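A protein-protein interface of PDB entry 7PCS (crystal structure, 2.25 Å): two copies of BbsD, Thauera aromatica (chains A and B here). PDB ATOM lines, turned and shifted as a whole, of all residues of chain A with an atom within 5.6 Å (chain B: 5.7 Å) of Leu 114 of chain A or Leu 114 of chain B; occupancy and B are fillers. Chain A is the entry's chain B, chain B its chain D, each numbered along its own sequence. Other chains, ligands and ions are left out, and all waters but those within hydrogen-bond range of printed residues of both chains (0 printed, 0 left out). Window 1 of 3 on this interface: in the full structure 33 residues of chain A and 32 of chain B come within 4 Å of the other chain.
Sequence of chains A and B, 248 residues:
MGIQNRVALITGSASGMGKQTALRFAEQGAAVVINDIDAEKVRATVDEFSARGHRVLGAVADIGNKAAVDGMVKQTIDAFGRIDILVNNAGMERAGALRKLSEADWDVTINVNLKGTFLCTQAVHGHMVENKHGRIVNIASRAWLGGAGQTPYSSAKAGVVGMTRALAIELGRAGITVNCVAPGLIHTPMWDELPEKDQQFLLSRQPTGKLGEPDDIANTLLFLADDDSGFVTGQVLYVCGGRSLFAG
Leu 114 of chain A touches just these residues of chain B: Trp 106 (3.7 Å), Ile 110 (3.9 Å) and Leu 114 (3.9 Å). Leu 114 of chain B touches just these residues of chain A: Trp 106 (3.7 Å), Ile 110 (3.9 Å) and Leu 114 (3.9 Å). Of the printed residues of chain A, Trp 106 of chain B touches Leu 114 (3.7 Å), Lys 115 (3.4 Å), Phe 118 (3.5 Å) and Met 163 (3.8 Å). Of the printed residues of chain B, Ser 155 of chain A touches Gly 159 (3.3 Å) and Met 163 (3.3 Å). Of the printed residues of chain A, Met 163 of chain B touches Trp 106 (3.9 Å) and Ser 155 (3.3 Å). Of the printed residues of chain B, Gly 159 of chain A touches Ser 155 (3.2 Å) and Gly 159 (3.7 Å). Of the printed residues of chain A, Ser 155 of chain B touches Gly 159 (3.2 Å) and Met 163 (3.3 Å). Thr 109 of chain B touches none of the printed residues of chain A. The nearest residue of chain B that does not touch Leu 114 of chain A is Ser 155 of chain B (4.2 Å).
Trp 106 of chain A touches Leu 114 of chain B, and with the chains exchanged Leu 114 of chain A touches Trp 106 of chain B. Ser 155 of chain A touches Gly 159 of chain B, and with the chains exchanged Gly 159 of chain A touches Ser 155 of chain B. Ser 155 of chain A touches Met 163 of chain B, and with the chains exchanged Met 163 of chain A touches Ser 155 of chain B. Gly 159 of chain B touches its own counterpart, Gly 159 of chain A. Of the 16 pairs that touch across the chains among the printed residues, 16 have their exchanged pair printed and touching as well.
Among the printed residues, merely in contact across the chains: Trp 106 of chain A with Leu 114 of chain B, Trp 106 of chain A with Lys 115 of chain B, Trp 106 of chain A with Phe 118 of chain B, Trp 106 of chain A with Met 163 of chain B, Ile 110 of chain A with Leu 114 of chain B, Leu 114 of chain A with Trp 106 of chain B, Leu 114 of chain A with Ile 110 of chain B, Leu 114 of chain A with Leu 114 of chain B, Lys 115 of chain A with Trp 106 of chain B, Phe 118 of chain A with Trp 106 of chain B, Ser 155 of chain A with Gly 159 of chain B, Ser 155 of chain A with Met 163 of chain B, Gly 159 of chain A with Ser 155 of chain B, Gly 159 of chain A with Gly 159 of chain B, Met 163 of chain A with Trp 106 of chain B and Met 163 of chain A with Ser 155 of chain B.
Printed residues of chain B that touch a printed residue of chain A: Trp 106, Ile 110, Leu 114, Lys 115, Phe 118, Ser 155, Gly 159 and Met 163. Hydrophobic or aromatic side chains of chain B within 4 Å of the printed part of chain A: Trp 106, Ile 110, Leu 114, Phe 118 and Met 163. Hydrophobic or aromatic side chains of chain A that line the printed part of chain B: Trp 106, Ile 110, Leu 114, Phe 118 and Met 163. Among the printed residues, 16 pairs touch across the chains.
O of Ile 110 of chain B is in hydrogen-bond range of N of Lys 115 of chain B, 3.0 Å away. O of Ile 110 of chain A sits at hydrogen-bond distance from N of Lys 115 of chain A (3.1 Å).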
ATOM      1  N   TRP A 106      -2.622  17.846  19.962  1.00  0.00           N
ATOM      2  CA  TRP A 106      -3.603  16.777  19.835  1.00  0.00           C
ATOM      3  C   TRP A 106      -4.342  16.863  18.503  1.00  0.00           C
ATOM      4  O   TRP A 106      -4.450  15.870  17.775  1.00  0.00           O
ATOM      5  CB  TRP A 106      -4.593  16.840  21.004  1.00  0.00           C
ATOM      6  CG  TRP A 106      -5.796  15.981  20.789  1.00  0.00           C
ATOM      7  CD1 TRP A 106      -6.972  16.343  20.190  1.00  0.00           C
ATOM      8  CD2 TRP A 106      -5.939  14.602  21.155  1.00  0.00           C
ATOM      9  NE1 TRP A 106      -7.830  15.269  20.153  1.00  0.00           N
ATOM     10  CE2 TRP A 106      -7.221  14.190  20.742  1.00  0.00           C
ATOM     11  CE3 TRP A 106      -5.102  13.674  21.784  1.00  0.00           C
ATOM     12  CZ2 TRP A 106      -7.686  12.887  20.942  1.00  0.00           C
ATOM     13  CZ3 TRP A 106      -5.568  12.387  21.989  1.00  0.00           C
ATOM     14  CH2 TRP A 106      -6.845  12.005  21.568  1.00  0.00           C
ATOM     15  N   THR A 109      -2.211  15.693  15.262  1.00  0.00           N
ATOM     16  CA  THR A 109      -1.882  14.274  15.214  1.00  0.00           C
ATOM     17  C   THR A 109      -3.118  13.455  14.869  1.00  0.00           C
ATOM     18  O   THR A 109      -3.053  12.531  14.048  1.00  0.00           O
ATOM     19  CB  THR A 109      -1.285  13.829  16.555  1.00  0.00           C
ATOM     20  OG1 THR A 109      -0.209  14.709  16.917  1.00  0.00           O
ATOM     21  CG2 THR A 109      -0.778  12.404  16.473  1.00  0.00           C
ATOM     22  N   ILE A 110      -4.261  13.798  15.471  1.00  0.00           N
ATOM     23  CA  ILE A 110      -5.511  13.115  15.151  1.00  0.00           C
ATOM     24  C   ILE A 110      -5.901  13.383  13.706  1.00  0.00           C
ATOM     25  O   ILE A 110      -6.293  12.466  12.971  1.00  0.00           O
ATOM     26  CB  ILE A 110      -6.621  13.555  16.124  1.00  0.00           C
ATOM     27  CG1 ILE A 110      -6.294  13.087  17.542  1.00  0.00           C
ATOM     28  CG2 ILE A 110      -7.979  13.049  15.640  1.00  0.00           C
ATOM     29  CD1 ILE A 110      -6.295  11.603  17.727  1.00  0.00           C
ATOM     30  N   ASN A 111      -5.771  14.637  13.268  1.00  0.00           N
ATOM     31  CA  ASN A 111      -6.252  15.027  11.947  1.00  0.00           C
ATOM     32  C   ASN A 111      -5.485  14.308  10.841  1.00  0.00           C
ATOM     33  O   ASN A 111      -6.084  13.729   9.926  1.00  0.00           O
ATOM     34  CB  ASN A 111      -6.142  16.549  11.799  1.00  0.00           C
ATOM     35  CG  ASN A 111      -6.790  17.062  10.535  1.00  0.00           C
ATOM     36  OD1 ASN A 111      -8.017  17.007  10.391  1.00  0.00           O
ATOM     37  ND2 ASN A 111      -5.971  17.593   9.615  1.00  0.00           N
ATOM     38  N   VAL A 112      -4.159  14.311  10.910  1.00  0.00           N
ATOM     39  CA  VAL A 112      -3.381  13.713   9.830  1.00  0.00           C
ATOM     40  C   VAL A 112      -3.513  12.196   9.845  1.00  0.00           C
ATOM     41  O   VAL A 112      -3.820  11.576   8.820  1.00  0.00           O
ATOM     42  CB  VAL A 112      -1.908  14.144   9.919  1.00  0.00           C
ATOM     43  CG1 VAL A 112      -1.100  13.524   8.777  1.00  0.00           C
ATOM     44  CG2 VAL A 112      -1.798  15.669   9.895  1.00  0.00           C
ATOM     45  N   ASN A 113      -3.267  11.573  11.000  1.00  0.00           N
ATOM     46  CA  ASN A 113      -3.186  10.115  11.049  1.00  0.00           C
ATOM     47  C   ASN A 113      -4.564   9.468  10.949  1.00  0.00           C
ATOM     48  O   ASN A 113      -4.784   8.575  10.120  1.00  0.00           O
ATOM     49  CB  ASN A 113      -2.478   9.678  12.332  1.00  0.00           C
ATOM     50  CG  ASN A 113      -1.003  10.059  12.349  1.00  0.00           C
ATOM     51  OD1 ASN A 113      -0.163   9.355  11.782  1.00  0.00           O
ATOM     52  ND2 ASN A 113      -0.681  11.167  13.010  1.00  0.00           N
ATOM     53  N   LEU A 114      -5.505   9.894  11.788  1.00  0.00           N
ATOM     54  CA  LEU A 114      -6.778   9.192  11.897  1.00  0.00           C
ATOM     55  C   LEU A 114      -7.809   9.720  10.903  1.00  0.00           C
ATOM     56  O   LEU A 114      -8.315   8.962  10.071  1.00  0.00           O
ATOM     57  CB  LEU A 114      -7.312   9.294  13.328  1.00  0.00           C
ATOM     58  CG  LEU A 114      -8.578   8.499  13.656  1.00  0.00           C
ATOM     59  CD1 LEU A 114      -8.384   7.035  13.351  1.00  0.00           C
ATOM     60  CD2 LEU A 114      -8.960   8.702  15.117  1.00  0.00           C
ATOM     61  N   LYS A 115      -8.142  11.010  10.980  1.00  0.00           N
ATOM     62  CA  LYS A 115      -9.112  11.566  10.037  1.00  0.00           C
ATOM     63  C   LYS A 115      -8.602  11.483   8.602  1.00  0.00           C
ATOM     64  O   LYS A 115      -9.363  11.168   7.679  1.00  0.00           O
ATOM     65  CB  LYS A 115      -9.429  13.019  10.393  1.00  0.00           C
ATOM     66  CG  LYS A 115     -10.482  13.650   9.495  1.00  0.00           C
ATOM     67  CD  LYS A 115     -10.849  15.069   9.951  1.00  0.00           C
ATOM     68  CE  LYS A 115     -12.009  15.626   9.126  1.00  0.00           C
ATOM     69  NZ  LYS A 115     -12.349  17.047   9.471  1.00  0.00           N
ATOM     70  N   GLY A 116      -7.326  11.814   8.387  1.00  0.00           N
ATOM     71  CA  GLY A 116      -6.769  11.710   7.048  1.00  0.00           C
ATOM     72  C   GLY A 116      -6.970  10.331   6.455  1.00  0.00           C
ATOM     73  O   GLY A 116      -7.370  10.183   5.296  1.00  0.00           O
ATOM     74  N   THR A 117      -6.695   9.297   7.250  1.00  0.00           N
ATOM     75  CA  THR A 117      -6.930   7.932   6.794  1.00  0.00           C
ATOM     76  C   THR A 117      -8.409   7.694   6.532  1.00  0.00           C
ATOM     77  O   THR A 117      -8.777   6.981   5.591  1.00  0.00           O
ATOM     78  CB  THR A 117      -6.396   6.942   7.828  1.00  0.00           C
ATOM     79  OG1 THR A 117      -4.967   6.915   7.743  1.00  0.00           O
ATOM     80  CG2 THR A 117      -6.947   5.544   7.578  1.00  0.00           C
ATOM     81  N   PHE A 118      -9.274   8.293   7.346  1.00  0.00           N
ATOM     82  CA  PHE A 118     -10.701   8.181   7.083  1.00  0.00           C
ATOM     83  C   PHE A 118     -11.086   8.912   5.803  1.00  0.00           C
ATOM     84  O   PHE A 118     -11.881   8.400   5.003  1.00  0.00           O
ATOM     85  CB  PHE A 118     -11.498   8.731   8.263  1.00  0.00           C
ATOM     86  CG  PHE A 118     -12.929   9.024   7.928  1.00  0.00           C
ATOM     87  CD1 PHE A 118     -13.866   8.005   7.864  1.00  0.00           C
ATOM     88  CD2 PHE A 118     -13.335  10.318   7.674  1.00  0.00           C
ATOM     89  CE1 PHE A 118     -15.186   8.280   7.551  1.00  0.00           C
ATOM     90  CE2 PHE A 118     -14.650  10.598   7.367  1.00  0.00           C
ATOM     91  CZ  PHE A 118     -15.576   9.578   7.303  1.00  0.00           C
ATOM     92  N   LEU A 119     -10.537  10.110   5.592  1.00  0.00           N
ATOM     93  CA  LEU A 119     -10.920  10.895   4.420  1.00  0.00           C
ATOM     94  C   LEU A 119     -10.503  10.193   3.135  1.00  0.00           C
ATOM     95  O   LEU A 119     -11.281  10.110   2.180  1.00  0.00           O
ATOM     96  CB  LEU A 119     -10.290  12.284   4.479  1.00  0.00           C
ATOM     97  CG  LEU A 119     -10.798  13.254   5.536  1.00  0.00           C
ATOM     98  CD1 LEU A 119     -10.001  14.558   5.458  1.00  0.00           C
ATOM     99  CD2 LEU A 119     -12.275  13.512   5.349  1.00  0.00           C
ATOM    100  N   SER A 155      -3.407   7.331  20.497  1.00  0.00           N
ATOM    101  CA  SER A 155      -4.837   7.451  20.238  1.00  0.00           C
ATOM    102  C   SER A 155      -5.133   7.368  18.748  1.00  0.00           C
ATOM    103  O   SER A 155      -6.017   6.618  18.317  1.00  0.00           O
ATOM    104  CB  SER A 155      -5.370   8.774  20.796  1.00  0.00           C
ATOM    105  OG  SER A 155      -5.166   8.876  22.187  1.00  0.00           O
ATOM    106  N   ALA A 156      -4.405   8.147  17.941  1.00  0.00           N
ATOM    107  CA  ALA A 156      -4.691   8.206  16.511  1.00  0.00           C
ATOM    108  C   ALA A 156      -4.474   6.852  15.842  1.00  0.00           C
ATOM    109  O   ALA A 156      -5.338   6.364  15.105  1.00  0.00           O
ATOM    110  CB  ALA A 156      -3.826   9.279  15.848  1.00  0.00           C
ATOM    111  N   GLY A 159      -6.943   4.342  16.756  1.00  0.00           N
ATOM    112  CA  GLY A 159      -8.154   4.610  15.995  1.00  0.00           C
ATOM    113  C   GLY A 159      -8.078   4.052  14.587  1.00  0.00           C
ATOM    114  O   GLY A 159      -9.069   3.553  14.048  1.00  0.00           O
ATOM    115  N   VAL A 160      -6.894   4.115  13.977  1.00  0.00           N
ATOM    116  CA  VAL A 160      -6.707   3.530  12.656  1.00  0.00           C
ATOM    117  C   VAL A 160      -6.932   2.028  12.706  1.00  0.00           C
ATOM    118  O   VAL A 160      -7.428   1.435  11.742  1.00  0.00           O
ATOM    119  CB  VAL A 160      -5.308   3.882  12.115  1.00  0.00           C
ATOM    120  CG1 VAL A 160      -4.937   2.982  10.929  1.00  0.00           C
ATOM    121  CG2 VAL A 160      -5.262   5.371  11.718  1.00  0.00           C
ATOM    122  N   MET A 163     -10.699   1.506  12.747  1.00  0.00           N
ATOM    123  CA  MET A 163     -11.223   1.769  11.413  1.00  0.00           C
ATOM    124  C   MET A 163     -10.939   0.600  10.485  1.00  0.00           C
ATOM    125  O   MET A 163     -11.801   0.203   9.692  1.00  0.00           O
ATOM    126  CB  MET A 163     -10.623   3.061  10.860  1.00  0.00           C
ATOM    127  CG  MET A 163     -11.501   3.786   9.864  1.00  0.00           C
ATOM    128  SD  MET A 163     -10.593   4.949   8.825  1.00  0.00           S
ATOM    129  CE  MET A 163      -9.932   6.050  10.067  1.00  0.00           C
ATOM    130  N   TRP B 106     -18.273  12.414  11.245  1.00  0.00           N
ATOM    131  CA  TRP B 106     -16.986  11.957  11.756  1.00  0.00           C
ATOM    132  C   TRP B 106     -16.489  12.873  12.867  1.00  0.00           C
ATOM    133  O   TRP B 106     -16.134  12.412  13.961  1.00  0.00           O
ATOM    134  CB  TRP B 106     -15.964  11.891  10.609  1.00  0.00           C
ATOM    135  CG  TRP B 106     -14.557  11.743  11.089  1.00  0.00           C
ATOM    136  CD1 TRP B 106     -13.690  12.748  11.395  1.00  0.00           C
ATOM    137  CD2 TRP B 106     -13.851  10.518  11.326  1.00  0.00           C
ATOM    138  NE1 TRP B 106     -12.492  12.227  11.822  1.00  0.00           N
ATOM    139  CE2 TRP B 106     -12.562  10.860  11.784  1.00  0.00           C
ATOM    140  CE3 TRP B 106     -14.183   9.166  11.199  1.00  0.00           C
ATOM    141  CZ2 TRP B 106     -11.612   9.904  12.121  1.00  0.00           C
ATOM    142  CZ3 TRP B 106     -13.236   8.216  11.525  1.00  0.00           C
ATOM    143  CH2 TRP B 106     -11.962   8.589  11.974  1.00  0.00           C
ATOM    144  N   THR B 109     -18.332  12.532  16.439  1.00  0.00           N
ATOM    145  CA  THR B 109     -18.092  11.265  17.120  1.00  0.00           C
ATOM    146  C   THR B 109     -16.686  11.225  17.691  1.00  0.00           C
ATOM    147  O   THR B 109     -16.483  10.801  18.833  1.00  0.00           O
ATOM    148  CB  THR B 109     -18.317  10.104  16.151  1.00  0.00           C
ATOM    149  OG1 THR B 109     -19.592  10.257  15.516  1.00  0.00           O
ATOM    150  CG2 THR B 109     -18.294   8.768  16.875  1.00  0.00           C
ATOM    151  N   ILE B 110     -15.704  11.684  16.913  1.00  0.00           N
ATOM    152  CA  ILE B 110     -14.329  11.753  17.400  1.00  0.00           C
ATOM    153  C   ILE B 110     -14.213  12.764  18.530  1.00  0.00           C
ATOM    154  O   ILE B 110     -13.561  12.505  19.551  1.00  0.00           O
ATOM    155  CB  ILE B 110     -13.372  12.097  16.241  1.00  0.00           C
ATOM    156  CG1 ILE B 110     -13.320  10.952  15.225  1.00  0.00           C
ATOM    157  CG2 ILE B 110     -11.983  12.442  16.777  1.00  0.00           C
ATOM    158  CD1 ILE B 110     -12.715   9.708  15.744  1.00  0.00           C
ATOM    159  N   ASN B 111     -14.842  13.930  18.368  1.00  0.00           N
ATOM    160  CA  ASN B 111     -14.672  15.009  19.332  1.00  0.00           C
ATOM    161  C   ASN B 111     -15.215  14.612  20.697  1.00  0.00           C
ATOM    162  O   ASN B 111     -14.554  14.809  21.721  1.00  0.00           O
ATOM    163  CB  ASN B 111     -15.358  16.277  18.819  1.00  0.00           C
ATOM    164  CG  ASN B 111     -15.065  17.490  19.685  1.00  0.00           C
ATOM    165  OD1 ASN B 111     -13.928  17.974  19.724  1.00  0.00           O
ATOM    166  ND2 ASN B 111     -16.087  17.989  20.384  1.00  0.00           N
ATOM    167  N   VAL B 112     -16.422  14.051  20.736  1.00  0.00           N
ATOM    168  CA  VAL B 112     -17.032  13.721  22.020  1.00  0.00           C
ATOM    169  C   VAL B 112     -16.317  12.537  22.665  1.00  0.00           C
ATOM    170  O   VAL B 112     -15.902  12.597  23.830  1.00  0.00           O
ATOM    171  CB  VAL B 112     -18.534  13.439  21.843  1.00  0.00           C
ATOM    172  CG1 VAL B 112     -19.179  13.162  23.200  1.00  0.00           C
ATOM    173  CG2 VAL B 112     -19.222  14.599  21.135  1.00  0.00           C
ATOM    174  N   ASN B 113     -16.171  11.438  21.921  1.00  0.00           N
ATOM    175  CA  ASN B 113     -15.667  10.200  22.503  1.00  0.00           C
ATOM    176  C   ASN B 113     -14.159  10.260  22.732  1.00  0.00           C
ATOM    177  O   ASN B 113     -13.677   9.979  23.835  1.00  0.00           O
ATOM    178  CB  ASN B 113     -16.014   9.013  21.598  1.00  0.00           C
ATOM    179  CG  ASN B 113     -17.504   8.747  21.524  1.00  0.00           C
ATOM    180  OD1 ASN B 113     -18.074   8.098  22.396  1.00  0.00           O
ATOM    181  ND2 ASN B 113     -18.140   9.243  20.474  1.00  0.00           N
ATOM    182  N   LEU B 114     -13.402  10.624  21.700  1.00  0.00           N
ATOM    183  CA  LEU B 114     -11.948  10.515  21.751  1.00  0.00           C
ATOM    184  C   LEU B 114     -11.305  11.768  22.335  1.00  0.00           C
ATOM    185  O   LEU B 114     -10.592  11.693  23.341  1.00  0.00           O
ATOM    186  CB  LEU B 114     -11.395  10.227  20.350  1.00  0.00           C
ATOM    187  CG  LEU B 114      -9.883   9.986  20.284  1.00  0.00           C
ATOM    188  CD1 LEU B 114      -9.469   8.881  21.214  1.00  0.00           C
ATOM    189  CD2 LEU B 114      -9.444   9.656  18.863  1.00  0.00           C
ATOM    190  N   LYS B 115     -11.531  12.924  21.705  1.00  0.00           N
ATOM    191  CA  LYS B 115     -10.955  14.157  22.231  1.00  0.00           C
ATOM    192  C   LYS B 115     -11.518  14.472  23.609  1.00  0.00           C
ATOM    193  O   LYS B 115     -10.775  14.852  24.520  1.00  0.00           O
ATOM    194  CB  LYS B 115     -11.211  15.327  21.281  1.00  0.00           C
ATOM    195  CG  LYS B 115     -10.539  16.617  21.729  1.00  0.00           C
ATOM    196  CD  LYS B 115     -10.706  17.735  20.712  1.00  0.00           C
ATOM    197  CE  LYS B 115      -9.867  18.942  21.099  1.00  0.00           C
ATOM    198  NZ  LYS B 115     -10.070  20.100  20.176  1.00  0.00           N
ATOM    199  N   GLY B 116     -12.833  14.330  23.778  1.00  0.00           N
ATOM    200  CA  GLY B 116     -13.431  14.575  25.080  1.00  0.00           C
ATOM    201  C   GLY B 116     -12.775  13.771  26.186  1.00  0.00           C
ATOM    202  O   GLY B 116     -12.479  14.291  27.263  1.00  0.00           O
ATOM    203  N   THR B 117     -12.548  12.480  25.941  1.00  0.00           N
ATOM    204  CA  THR B 117     -11.852  11.664  26.931  1.00  0.00           C
ATOM    205  C   THR B 117     -10.428  12.159  27.150  1.00  0.00           C
ATOM    206  O   THR B 117      -9.907  12.103  28.270  1.00  0.00           O
ATOM    207  CB  THR B 117     -11.859  10.202  26.491  1.00  0.00           C
ATOM    208  OG1 THR B 117     -13.168   9.664  26.703  1.00  0.00           O
ATOM    209  CG2 THR B 117     -10.828   9.394  27.260  1.00  0.00           C
ATOM    210  N   PHE B 118      -9.780  12.647  26.088  1.00  0.00           N
ATOM    211  CA  PHE B 118      -8.440  13.205  26.247  1.00  0.00           C
ATOM    212  C   PHE B 118      -8.472  14.491  27.067  1.00  0.00           C
ATOM    213  O   PHE B 118      -7.611  14.707  27.929  1.00  0.00           O
ATOM    214  CB  PHE B 118      -7.802  13.465  24.879  1.00  0.00           C
ATOM    215  CG  PHE B 118      -6.594  14.365  24.938  1.00  0.00           C
ATOM    216  CD1 PHE B 118      -5.367  13.867  25.332  1.00  0.00           C
ATOM    217  CD2 PHE B 118      -6.691  15.706  24.604  1.00  0.00           C
ATOM    218  CE1 PHE B 118      -4.264  14.686  25.402  1.00  0.00           C
ATOM    219  CE2 PHE B 118      -5.584  16.533  24.658  1.00  0.00           C
ATOM    220  CZ  PHE B 118      -4.370  16.024  25.062  1.00  0.00           C
ATOM    221  N   LEU B 119      -9.451  15.358  26.813  1.00  0.00           N
ATOM    222  CA  LEU B 119      -9.495  16.642  27.506  1.00  0.00           C
ATOM    223  C   LEU B 119      -9.728  16.456  29.000  1.00  0.00           C
ATOM    224  O   LEU B 119      -9.054  17.080  29.825  1.00  0.00           O
ATOM    225  CB  LEU B 119     -10.582  17.527  26.904  1.00  0.00           C
ATOM    226  CG  LEU B 119     -10.327  18.028  25.482  1.00  0.00           C
ATOM    227  CD1 LEU B 119     -11.501  18.894  25.021  1.00  0.00           C
ATOM    228  CD2 LEU B 119      -9.024  18.794  25.406  1.00  0.00           C
ATOM    229  N   SER B 155     -13.607   3.882  15.181  1.00  0.00           N
ATOM    230  CA  SER B 155     -12.355   4.633  15.196  1.00  0.00           C
ATOM    231  C   SER B 155     -12.175   5.360  16.520  1.00  0.00           C
ATOM    232  O   SER B 155     -11.113   5.281  17.151  1.00  0.00           O
ATOM    233  CB  SER B 155     -12.321   5.622  14.031  1.00  0.00           C
ATOM    234  OG  SER B 155     -12.442   4.960  12.786  1.00  0.00           O
ATOM    235  N   ALA B 156     -13.213   6.074  16.958  1.00  0.00           N
ATOM    236  CA  ALA B 156     -13.107   6.868  18.177  1.00  0.00           C
ATOM    237  C   ALA B 156     -12.839   5.981  19.386  1.00  0.00           C
ATOM    238  O   ALA B 156     -11.936   6.258  20.186  1.00  0.00           O
ATOM    239  CB  ALA B 156     -14.381   7.688  18.389  1.00  0.00           C
ATOM    240  N   GLY B 159      -9.493   4.439  19.483  1.00  0.00           N
ATOM    241  CA  GLY B 159      -8.561   5.443  19.967  1.00  0.00           C
ATOM    242  C   GLY B 159      -8.565   5.553  21.478  1.00  0.00           C
ATOM    243  O   GLY B 159      -7.520   5.768  22.094  1.00  0.00           O
ATOM    244  N   VAL B 160      -9.737   5.394  22.100  1.00  0.00           N
ATOM    245  CA  VAL B 160      -9.805   5.413  23.559  1.00  0.00           C
ATOM    246  C   VAL B 160      -9.009   4.256  24.150  1.00  0.00           C
ATOM    247  O   VAL B 160      -8.424   4.382  25.231  1.00  0.00           O
ATOM    248  CB  VAL B 160     -11.274   5.379  24.027  1.00  0.00           C
ATOM    249  CG1 VAL B 160     -11.367   5.052  25.513  1.00  0.00           C
ATOM    250  CG2 VAL B 160     -11.956   6.718  23.717  1.00  0.00           C
ATOM    251  N   MET B 163      -5.334   5.250  23.950  1.00  0.00           N
ATOM    252  CA  MET B 163      -5.082   6.238  24.989  1.00  0.00           C
ATOM    253  C   MET B 163      -4.996   5.575  26.357  1.00  0.00           C
ATOM    254  O   MET B 163      -4.127   5.913  27.171  1.00  0.00           O
ATOM    255  CB  MET B 163      -6.177   7.299  24.978  1.00  0.00           C
ATOM    256  CG  MET B 163      -5.700   8.653  25.464  1.00  0.00           C
ATOM    257  SD  MET B 163      -7.044   9.703  26.013  1.00  0.00           S
ATOM    258  CE  MET B 163      -8.039   9.811  24.519  1.00  0.00           C
